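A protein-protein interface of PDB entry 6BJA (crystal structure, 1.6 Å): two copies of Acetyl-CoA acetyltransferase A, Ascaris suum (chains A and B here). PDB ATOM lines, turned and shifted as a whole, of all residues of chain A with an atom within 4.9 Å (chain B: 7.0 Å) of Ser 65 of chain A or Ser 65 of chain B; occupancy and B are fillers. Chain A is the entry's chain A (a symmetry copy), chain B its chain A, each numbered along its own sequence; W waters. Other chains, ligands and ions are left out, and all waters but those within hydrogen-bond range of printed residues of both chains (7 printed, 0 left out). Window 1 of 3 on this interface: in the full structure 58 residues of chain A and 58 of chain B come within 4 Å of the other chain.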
ATOM      1  N   ASN A  62     -15.497  -6.894  -7.487  1.00  0.00           N
ATOM      2  CA  ASN A  62     -14.723  -7.917  -8.176  1.00  0.00           C
ATOM      3  C   ASN A  62     -15.562  -8.472  -9.301  1.00  0.00           C
ATOM      4  O   ASN A  62     -16.730  -8.754  -9.098  1.00  0.00           O
ATOM      5  CB  ASN A  62     -14.315  -9.045  -7.215  1.00  0.00           C
ATOM      6  CG  ASN A  62     -13.581 -10.167  -7.912  1.00  0.00           C
ATOM      7  OD1 ASN A  62     -14.153 -11.230  -8.207  1.00  0.00           O
ATOM      8  ND2 ASN A  62     -12.298  -9.956  -8.166  1.00  0.00           N
ATOM      9  N   VAL A  63     -14.975  -8.595 -10.483  1.00  0.00           N
ATOM     10  CA  VAL A  63     -15.686  -9.085 -11.656  1.00  0.00           C
ATOM     11  C   VAL A  63     -15.413 -10.570 -11.922  1.00  0.00           C
ATOM     12  O   VAL A  63     -16.352 -11.353 -12.089  1.00  0.00           O
ATOM     13  CB  VAL A  63     -15.315  -8.251 -12.893  1.00  0.00           C
ATOM     14  CG1 VAL A  63     -16.091  -8.744 -14.123  1.00  0.00           C
ATOM     15  CG2 VAL A  63     -15.572  -6.776 -12.617  1.00  0.00           C
ATOM     16  N   LEU A  64     -14.138 -10.954 -11.995  1.00  0.00           N
ATOM     17  CA  LEU A  64     -13.770 -12.300 -12.396  1.00  0.00           C
ATOM     18  C   LEU A  64     -13.547 -13.130 -11.144  1.00  0.00           C
ATOM     19  O   LEU A  64     -12.416 -13.379 -10.709  1.00  0.00           O
ATOM     20  CB  LEU A  64     -12.541 -12.267 -13.307  1.00  0.00           C
ATOM     21  CG  LEU A  64     -12.762 -11.396 -14.548  1.00  0.00           C
ATOM     22  CD1 LEU A  64     -11.461 -11.062 -15.213  1.00  0.00           C
ATOM     23  CD2 LEU A  64     -13.722 -12.078 -15.521  1.00  0.00           C
ATOM     24  N   SER A  65     -14.666 -13.572 -10.585  1.00  0.00           N
ATOM     25  CA  SER A  65     -14.644 -14.222  -9.279  1.00  0.00           C
ATOM     26  C   SER A  65     -14.376 -15.719  -9.371  1.00  0.00           C
ATOM     27  O   SER A  65     -14.284 -16.388  -8.340  1.00  0.00           O
ATOM     28  CB  SER A  65     -15.968 -13.974  -8.576  1.00  0.00           C
ATOM     29  OG  SER A  65     -17.027 -14.582  -9.299  1.00  0.00           O
ATOM     30  N   ALA A  66     -14.273 -16.264 -10.584  1.00  0.00           N
ATOM     31  CA  ALA A  66     -14.122 -17.721 -10.723  1.00  0.00           C
ATOM     32  C   ALA A  66     -12.830 -18.255 -10.109  1.00  0.00           C
ATOM     33  O   ALA A  66     -11.717 -17.801 -10.427  1.00  0.00           O
ATOM     34  CB  ALA A  66     -14.193 -18.130 -12.184  1.00  0.00           C
ATOM     35  N   GLY A  67     -12.993 -19.268  -9.259  1.00  0.00           N
ATOM     36  CA  GLY A  67     -11.871 -19.980  -8.682  1.00  0.00           C
ATOM     37  C   GLY A  67     -11.345 -19.364  -7.414  1.00  0.00           C
ATOM     38  O   GLY A  67     -10.398 -19.884  -6.826  1.00  0.00           O
ATOM     39  N   LEU A  68     -11.929 -18.247  -6.988  1.00  0.00           N
ATOM     40  CA  LEU A  68     -11.378 -17.502  -5.860  1.00  0.00           C
ATOM     41  C   LEU A  68     -11.939 -17.916  -4.507  1.00  0.00           C
ATOM     42  O   LEU A  68     -11.463 -17.457  -3.472  1.00  0.00           O
ATOM     43  CB  LEU A  68     -11.618 -16.018  -6.047  1.00  0.00           C
ATOM     44  CG  LEU A  68     -11.174 -15.502  -7.414  1.00  0.00           C
ATOM     45  CD1 LEU A  68     -11.243 -13.989  -7.412  1.00  0.00           C
ATOM     46  CD2 LEU A  68      -9.771 -15.992  -7.757  1.00  0.00           C
ATOM     47  N   GLY A  69     -12.958 -18.760  -4.516  1.00  0.00           N
ATOM     48  CA  GLY A  69     -13.541 -19.236  -3.277  1.00  0.00           C
ATOM     49  C   GLY A  69     -14.843 -18.545  -2.948  1.00  0.00           C
ATOM     50  O   GLY A  69     -15.366 -17.766  -3.737  1.00  0.00           O
ATOM     51  N   ASP A 151     -16.694 -13.282 -19.235  1.00  0.00           N
ATOM     52  CA  ASP A 151     -17.223 -12.620 -18.047  1.00  0.00           C
ATOM     53  C   ASP A 151     -16.661 -11.207 -17.831  1.00  0.00           C
ATOM     54  O   ASP A 151     -17.125 -10.486 -16.950  1.00  0.00           O
ATOM     55  CB  ASP A 151     -16.937 -13.490 -16.811  1.00  0.00           C
ATOM     56  CG  ASP A 151     -17.702 -14.824 -16.817  1.00  0.00           C
ATOM     57  OD1 ASP A 151     -18.717 -14.944 -17.532  1.00  0.00           O
ATOM     58  OD2 ASP A 151     -17.288 -15.749 -16.075  1.00  0.00           O
ATOM     59  N   ASN B  62     -26.417 -14.105  -6.721  1.00  0.00           N
ATOM     60  CA  ASN B  62     -25.890 -15.210  -7.511  1.00  0.00           C
ATOM     61  C   ASN B  62     -24.508 -15.541  -7.002  1.00  0.00           C
ATOM     62  O   ASN B  62     -23.718 -14.642  -6.775  1.00  0.00           O
ATOM     63  CB  ASN B  62     -25.830 -14.847  -9.003  1.00  0.00           C
ATOM     64  CG  ASN B  62     -25.209 -15.939  -9.843  1.00  0.00           C
ATOM     65  OD1 ASN B  62     -24.032 -15.865 -10.235  1.00  0.00           O
ATOM     66  ND2 ASN B  62     -25.998 -16.958 -10.152  1.00  0.00           N
ATOM     67  N   VAL B  63     -24.236 -16.823  -6.794  1.00  0.00           N
ATOM     68  CA  VAL B  63     -22.953 -17.269  -6.273  1.00  0.00           C
ATOM     69  C   VAL B  63     -22.015 -17.763  -7.382  1.00  0.00           C
ATOM     70  O   VAL B  63     -20.863 -17.330  -7.457  1.00  0.00           O
ATOM     71  CB  VAL B  63     -23.157 -18.375  -5.225  1.00  0.00           C
ATOM     72  CG1 VAL B  63     -21.806 -18.823  -4.647  1.00  0.00           C
ATOM     73  CG2 VAL B  63     -24.101 -17.886  -4.135  1.00  0.00           C
ATOM     74  N   LEU B  64     -22.490 -18.687  -8.217  1.00  0.00           N
ATOM     75  CA  LEU B  64     -21.639 -19.333  -9.200  1.00  0.00           C
ATOM     76  C   LEU B  64     -21.799 -18.607 -10.525  1.00  0.00           C
ATOM     77  O   LEU B  64     -22.509 -19.046 -11.438  1.00  0.00           O
ATOM     78  CB  LEU B  64     -21.978 -20.822  -9.301  1.00  0.00           C
ATOM     79  CG  LEU B  64     -21.851 -21.538  -7.952  1.00  0.00           C
ATOM     80  CD1 LEU B  64     -22.543 -22.868  -7.978  1.00  0.00           C
ATOM     81  CD2 LEU B  64     -20.384 -21.686  -7.556  1.00  0.00           C
ATOM     82  N   SER B  65     -21.095 -17.486 -10.611  1.00  0.00           N
ATOM     83  CA  SER B  65     -21.278 -16.574 -11.734  1.00  0.00           C
ATOM     84  C   SER B  65     -20.409 -16.935 -12.933  1.00  0.00           C
ATOM     85  O   SER B  65     -20.496 -16.275 -13.973  1.00  0.00           O
ATOM     86  CB  SER B  65     -20.973 -15.156 -11.282  1.00  0.00           C
ATOM     87  OG  SER B  65     -19.609 -15.046 -10.905  1.00  0.00           O
ATOM     88  N   ALA B  66     -19.556 -17.952 -12.806  1.00  0.00           N
ATOM     89  CA  ALA B  66     -18.623 -18.268 -13.899  1.00  0.00           C
ATOM     90  C   ALA B  66     -19.324 -18.701 -15.186  1.00  0.00           C
ATOM     91  O   ALA B  66     -20.142 -19.637 -15.202  1.00  0.00           O
ATOM     92  CB  ALA B  66     -17.643 -19.346 -13.471  1.00  0.00           C
ATOM     93  N   GLY B  67     -18.948 -18.035 -16.275  1.00  0.00           N
ATOM     94  CA  GLY B  67     -19.413 -18.399 -17.600  1.00  0.00           C
ATOM     95  C   GLY B  67     -20.713 -17.748 -17.988  1.00  0.00           C
ATOM     96  O   GLY B  67     -21.205 -17.972 -19.093  1.00  0.00           O
ATOM     97  N   LEU B  68     -21.296 -16.958 -17.090  1.00  0.00           N
ATOM     98  CA  LEU B  68     -22.632 -16.420 -17.326  1.00  0.00           C
ATOM     99  C   LEU B  68     -22.643 -15.069 -18.028  1.00  0.00           C
ATOM    100  O   LEU B  68     -23.703 -14.574 -18.399  1.00  0.00           O
ATOM    101  CB  LEU B  68     -23.380 -16.287 -16.015  1.00  0.00           C
ATOM    102  CG  LEU B  68     -23.360 -17.563 -15.176  1.00  0.00           C
ATOM    103  CD1 LEU B  68     -24.316 -17.399 -14.013  1.00  0.00           C
ATOM    104  CD2 LEU B  68     -23.717 -18.782 -16.021  1.00  0.00           C
ATOM    105  N   GLY B  69     -21.474 -14.469 -18.190  1.00  0.00           N
ATOM    106  CA  GLY B  69     -21.380 -13.195 -18.873  1.00  0.00           C
ATOM    107  C   GLY B  69     -21.208 -12.038 -17.919  1.00  0.00           C
ATOM    108  O   GLY B  69     -21.048 -12.225 -16.717  1.00  0.00           O
ATOM    109  N   ILE B  72     -24.939 -10.404 -14.467  1.00  0.00           N
ATOM    110  CA  ILE B  72     -26.184 -11.025 -14.928  1.00  0.00           C
ATOM    111  C   ILE B  72     -27.408 -10.191 -14.552  1.00  0.00           C
ATOM    112  O   ILE B  72     -28.414 -10.268 -15.249  1.00  0.00           O
ATOM    113  CB  ILE B  72     -26.374 -12.466 -14.402  1.00  0.00           C
ATOM    114  CG1 ILE B  72     -26.435 -12.518 -12.878  1.00  0.00           C
ATOM    115  CG2 ILE B  72     -25.299 -13.380 -14.963  1.00  0.00           C
ATOM    116  CD1 ILE B  72     -26.882 -13.848 -12.390  1.00  0.00           C
ATOM    117  N   THR B  90     -25.080  -7.338  -9.376  1.00  0.00           N
ATOM    118  CA  THR B  90     -25.094  -8.740  -8.973  1.00  0.00           C
ATOM    119  C   THR B  90     -24.284  -8.853  -7.704  1.00  0.00           C
ATOM    120  O   THR B  90     -23.209  -8.277  -7.597  1.00  0.00           O
ATOM    121  CB  THR B  90     -24.535  -9.673 -10.061  1.00  0.00           C
ATOM    122  OG1 THR B  90     -25.218  -9.414 -11.304  1.00  0.00           O
ATOM    123  CG2 THR B  90     -24.784 -11.126  -9.724  1.00  0.00           C
ATOM    124  N   ASN B  92     -22.856 -11.259  -4.231  1.00  0.00           N
ATOM    125  CA  ASN B  92     -22.478 -12.577  -3.735  1.00  0.00           C
ATOM    126  C   ASN B  92     -22.240 -12.491  -2.240  1.00  0.00           C
ATOM    127  O   ASN B  92     -21.285 -11.863  -1.797  1.00  0.00           O
ATOM    128  CB  ASN B  92     -21.218 -13.095  -4.446  1.00  0.00           C
ATOM    129  CG  ASN B  92     -20.797 -14.482  -3.991  1.00  0.00           C
ATOM    130  OD1 ASN B  92     -21.347 -15.034  -3.053  1.00  0.00           O
ATOM    131  ND2 ASN B  92     -19.795 -15.046  -4.656  1.00  0.00           N
ATOM    132  N   GLU B 123     -29.953 -19.147  -9.415  1.00  0.00           N
ATOM    133  CA  GLU B 123     -28.797 -20.012  -9.429  1.00  0.00           C
ATOM    134  C   GLU B 123     -29.061 -21.209 -10.304  1.00  0.00           C
ATOM    135  O   GLU B 123     -30.097 -21.871 -10.170  1.00  0.00           O
ATOM    136  CB  GLU B 123     -28.431 -20.467  -8.012  1.00  0.00           C
ATOM    137  CG  GLU B 123     -27.005 -20.986  -7.904  1.00  0.00           C
ATOM    138  CD  GLU B 123     -25.978 -19.855  -7.812  1.00  0.00           C
ATOM    139  OE1 GLU B 123     -26.128 -19.009  -6.900  1.00  0.00           O
ATOM    140  OE2 GLU B 123     -25.016 -19.832  -8.619  1.00  0.00           O
ATOM    141  N   PRO B 129     -19.319 -24.472 -14.153  1.00  0.00           N
ATOM    142  CA  PRO B 129     -18.311 -25.192 -14.928  1.00  0.00           C
ATOM    143  C   PRO B 129     -17.162 -25.734 -14.105  1.00  0.00           C
ATOM    144  O   PRO B 129     -17.178 -25.643 -12.882  1.00  0.00           O
ATOM    145  CB  PRO B 129     -17.804 -24.119 -15.881  1.00  0.00           C
ATOM    146  CG  PRO B 129     -17.808 -22.875 -15.005  1.00  0.00           C
ATOM    147  CD  PRO B 129     -19.097 -23.016 -14.191  1.00  0.00           C
ATOM    148  N   TYR B 131     -12.819 -25.437 -13.906  1.00  0.00           N
ATOM    149  CA  TYR B 131     -11.791 -24.448 -14.189  1.00  0.00           C
ATOM    150  C   TYR B 131     -10.464 -25.088 -14.573  1.00  0.00           C
ATOM    151  O   TYR B 131      -9.970 -25.977 -13.885  1.00  0.00           O
ATOM    152  CB  TYR B 131     -11.555 -23.562 -12.956  1.00  0.00           C
ATOM    153  CG  TYR B 131     -12.782 -22.896 -12.358  1.00  0.00           C
ATOM    154  CD1 TYR B 131     -13.762 -22.349 -13.172  1.00  0.00           C
ATOM    155  CD2 TYR B 131     -12.925 -22.768 -10.977  1.00  0.00           C
ATOM    156  CE1 TYR B 131     -14.851 -21.711 -12.634  1.00  0.00           C
ATOM    157  CE2 TYR B 131     -14.009 -22.134 -10.429  1.00  0.00           C
ATOM    158  CZ  TYR B 131     -14.976 -21.604 -11.268  1.00  0.00           C
ATOM    159  OH  TYR B 131     -16.066 -20.953 -10.744  1.00  0.00           O
ATOM    160  N   ASP B 151     -16.116 -22.601  -5.313  1.00  0.00           N
ATOM    161  CA  ASP B 151     -16.780 -21.312  -5.147  1.00  0.00           C
ATOM    162  C   ASP B 151     -18.145 -21.412  -4.450  1.00  0.00           C
ATOM    163  O   ASP B 151     -18.747 -20.391  -4.120  1.00  0.00           O
ATOM    164  CB  ASP B 151     -16.943 -20.642  -6.521  1.00  0.00           C
ATOM    165  CG  ASP B 151     -15.605 -20.246  -7.167  1.00  0.00           C
ATOM    166  OD1 ASP B 151     -14.593 -20.122  -6.448  1.00  0.00           O
ATOM    167  OD2 ASP B 151     -15.582 -20.035  -8.404  1.00  0.00           O
HETATM  168  O   HOH W   1     -19.876 -14.469  -7.923  1.00  0.00           O
HETATM  169  O   HOH W   2     -18.470 -17.663  -4.240  1.00  0.00           O
HETATM  170  O   HOH W   3     -17.458 -16.219 -11.078  1.00  0.00           O
HETATM  171  O   HOH W   4     -18.613 -12.131 -10.177  1.00  0.00           O
HETATM  172  O   HOH W   5     -19.033 -10.548 -14.977  1.00  0.00           O
HETATM  173  O   HOH W   6     -18.459 -12.759 -13.037  1.00  0.00           O
HETATM  174  O   HOH W   7     -18.245 -16.759  -7.090  1.00  0.00           O
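N of Leu 68 of chain B lies within hydrogen-bond range of OD1 of Asp 151 of chain A (3.3 Å). The side-chain carboxylate (OD1) of Asp 151 of chain B is in hydrogen-bond range of the backbone NH (N) of Gly 69 of chain A (2.9 Å). The side-chain carboxylate (OD1) of Asp 151 of chain A lies within hydrogen-bond range of the backbone NH (N) of Gly 69 of chain B (2.9 Å). The side-chain carboxylate (OD1) of Asp 151 of chain B is in hydrogen-bond range of the backbone NH (N) of Leu 68 of chain A (3.3 Å). The backbone NH (N) of Gly 67 of chain B lies within hydrogen-bond range of the side-chain carboxylate (OD2) of Asp 151 of chain A (2.8 Å). OG of Ser 65 of chain A sits at hydrogen-bond distance from OG of Ser 65 of chain B. The backbone NH (N) of Gly 67 of chain A sits at hydrogen-bond distance from the side-chain carboxylate (OD2) of Asp 151 of chain B, 2.8 Å away.
Ser 65 of chain A touches Asp 151 of chain B, and with the chains exchanged Asp 151 of chain A touches Ser 65 of chain B. Ala 66 of chain A touches its own counterpart, Ala 66 of chain B. Ala 66 of chain A touches Asp 151 of chain B, and with the chains exchanged Asp 151 of chain A touches Ala 66 of chain B. Leu 68 of chain A touches Asp 151 of chain B, and with the chains exchanged Asp 151 of chain A touches Leu 68 of chain B. 9 positions are printed for both chains.
Among the printed residues, pairs that only touch across the chains: Gly 67 of chain A with Tyr 131 of chain B, Asp 151 of chain A with Ala 66 of chain B, Ala 66 of chain A with Asp 151 of chain B, Ala 66 of chain A with Tyr 131 of chain B, Asp 151 of chain A with Ser 65 of chain B, Ser 65 of chain A with Asp 151 of chain B and Ala 66 of chain A with Ala 66 of chain B.
Of chain B, only Ser 65 (3.1 Å) and Asp 151 (3.9 Å) come within 4 Å of Ser 65 of chain A. Of the printed residues of chain B, Asp 151 of chain A touches Ser 65 (3.9 Å), Ala 66 (3.6 Å), Gly 67 (2.8 Å), Leu 68 (3.3 Å) and Gly 69 (2.9 Å). Val 63 of chain B touches none of the printed residues of chain A. Ser 65 of chain B touches just these residues of chain A: Ser 65 and Asp 151. Printed residues of chain A within 4 Å of Ala 66 of chain B: Ala 66 (3.9 Å) and Asp 151 (3.6 Å). Pro 129 of chain B touches none of the printed residues of chain A. Of the printed residues of chain A, Tyr 131 of chain B touches Ala 66 (3.7 Å) and Gly 67 (3.3 Å). The nearest residue of chain B that does not touch Ser 65 of chain A is Val 63 of chain B (5.1 Å). The nearest printed residue of chain A that does not touch Gly 67 of chain B is Ala 66 of chain A (6.3 Å).
Water W3 lies within hydrogen-bond range of the side-chain hydroxyl of Ser 65 of chain A (2.5 Å), the side-chain hydroxyl of Ser 65 of chain B (2.5 Å), the backbone NH of Ala 66 of chain A (3.2 Å) and the backbone NH of Ala 66 of chain B (3.2 Å). Water W7 lies within hydrogen-bond range of the backbone carbonyl oxygen (O) of Val 63 of chain B (2.7 Å), the side-chain hydroxyl (OG) of Ser 65 of chain A (3.3 Å) and the side-chain amide nitrogen (ND2) of Asn 92 of chain B (3.4 Å). Water W5 lies within hydrogen-bond range of the backbone carbonyl oxygen of Asp 151 of chain A and the backbone carbonyl oxygen of Gly 69 of chain B. Water W2 lies within hydrogen-bond range of O of Asp 151 of chain B (2.7 Å), ND2 of Asn 92 of chain B (3.0 Å) and O of Gly 69 of chain A (3.1 Å). Water W1 lies within hydrogen-bond range of the side-chain hydroxyl (OG) of Ser 65 of chain B (3.0 Å), the backbone carbonyl oxygen (O) of Val 63 of chain B (3.1 Å), the side-chain hydroxyl (OG) of Ser 65 of chain A (3.2 Å) and the side-chain amide nitrogen (ND2) of Asn 92 of chain B (3.3 Å). Water W4 lies within hydrogen-bond range of the side-chain hydroxyl of Ser 65 of chain A (3.0 Å), the backbone carbonyl oxygen of Val 63 of chain A (3.1 Å) and the side-chain hydroxyl of Ser 65 of chain B (3.2 Å).
Printed residues of chain B that touch a printed residue of chain A: Ser 65, Ala 66, Gly 67, Leu 68, Gly 69, Tyr 131 and Asp 151. Among the printed residues, no Asp or Glu carboxylate lies within 4 Å of a Lys or Arg side-chain nitrogen of the other chain.
The backbone NH (N) of Ser 65 of chain A sits close to the side-chain amide oxygen (OD1) of Asn 62 of chain A, 3.4 Å away. The side-chain carboxylate (OD2) of Asp 151 of chain B sits at hydrogen-bond distance from the side-chain hydroxyl (OH) of Tyr 131 of chain B, 2.6 Å away. OD1 of Asn 62 of chain B lies close to N of Ser 65 of chain B (3.4 Å).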
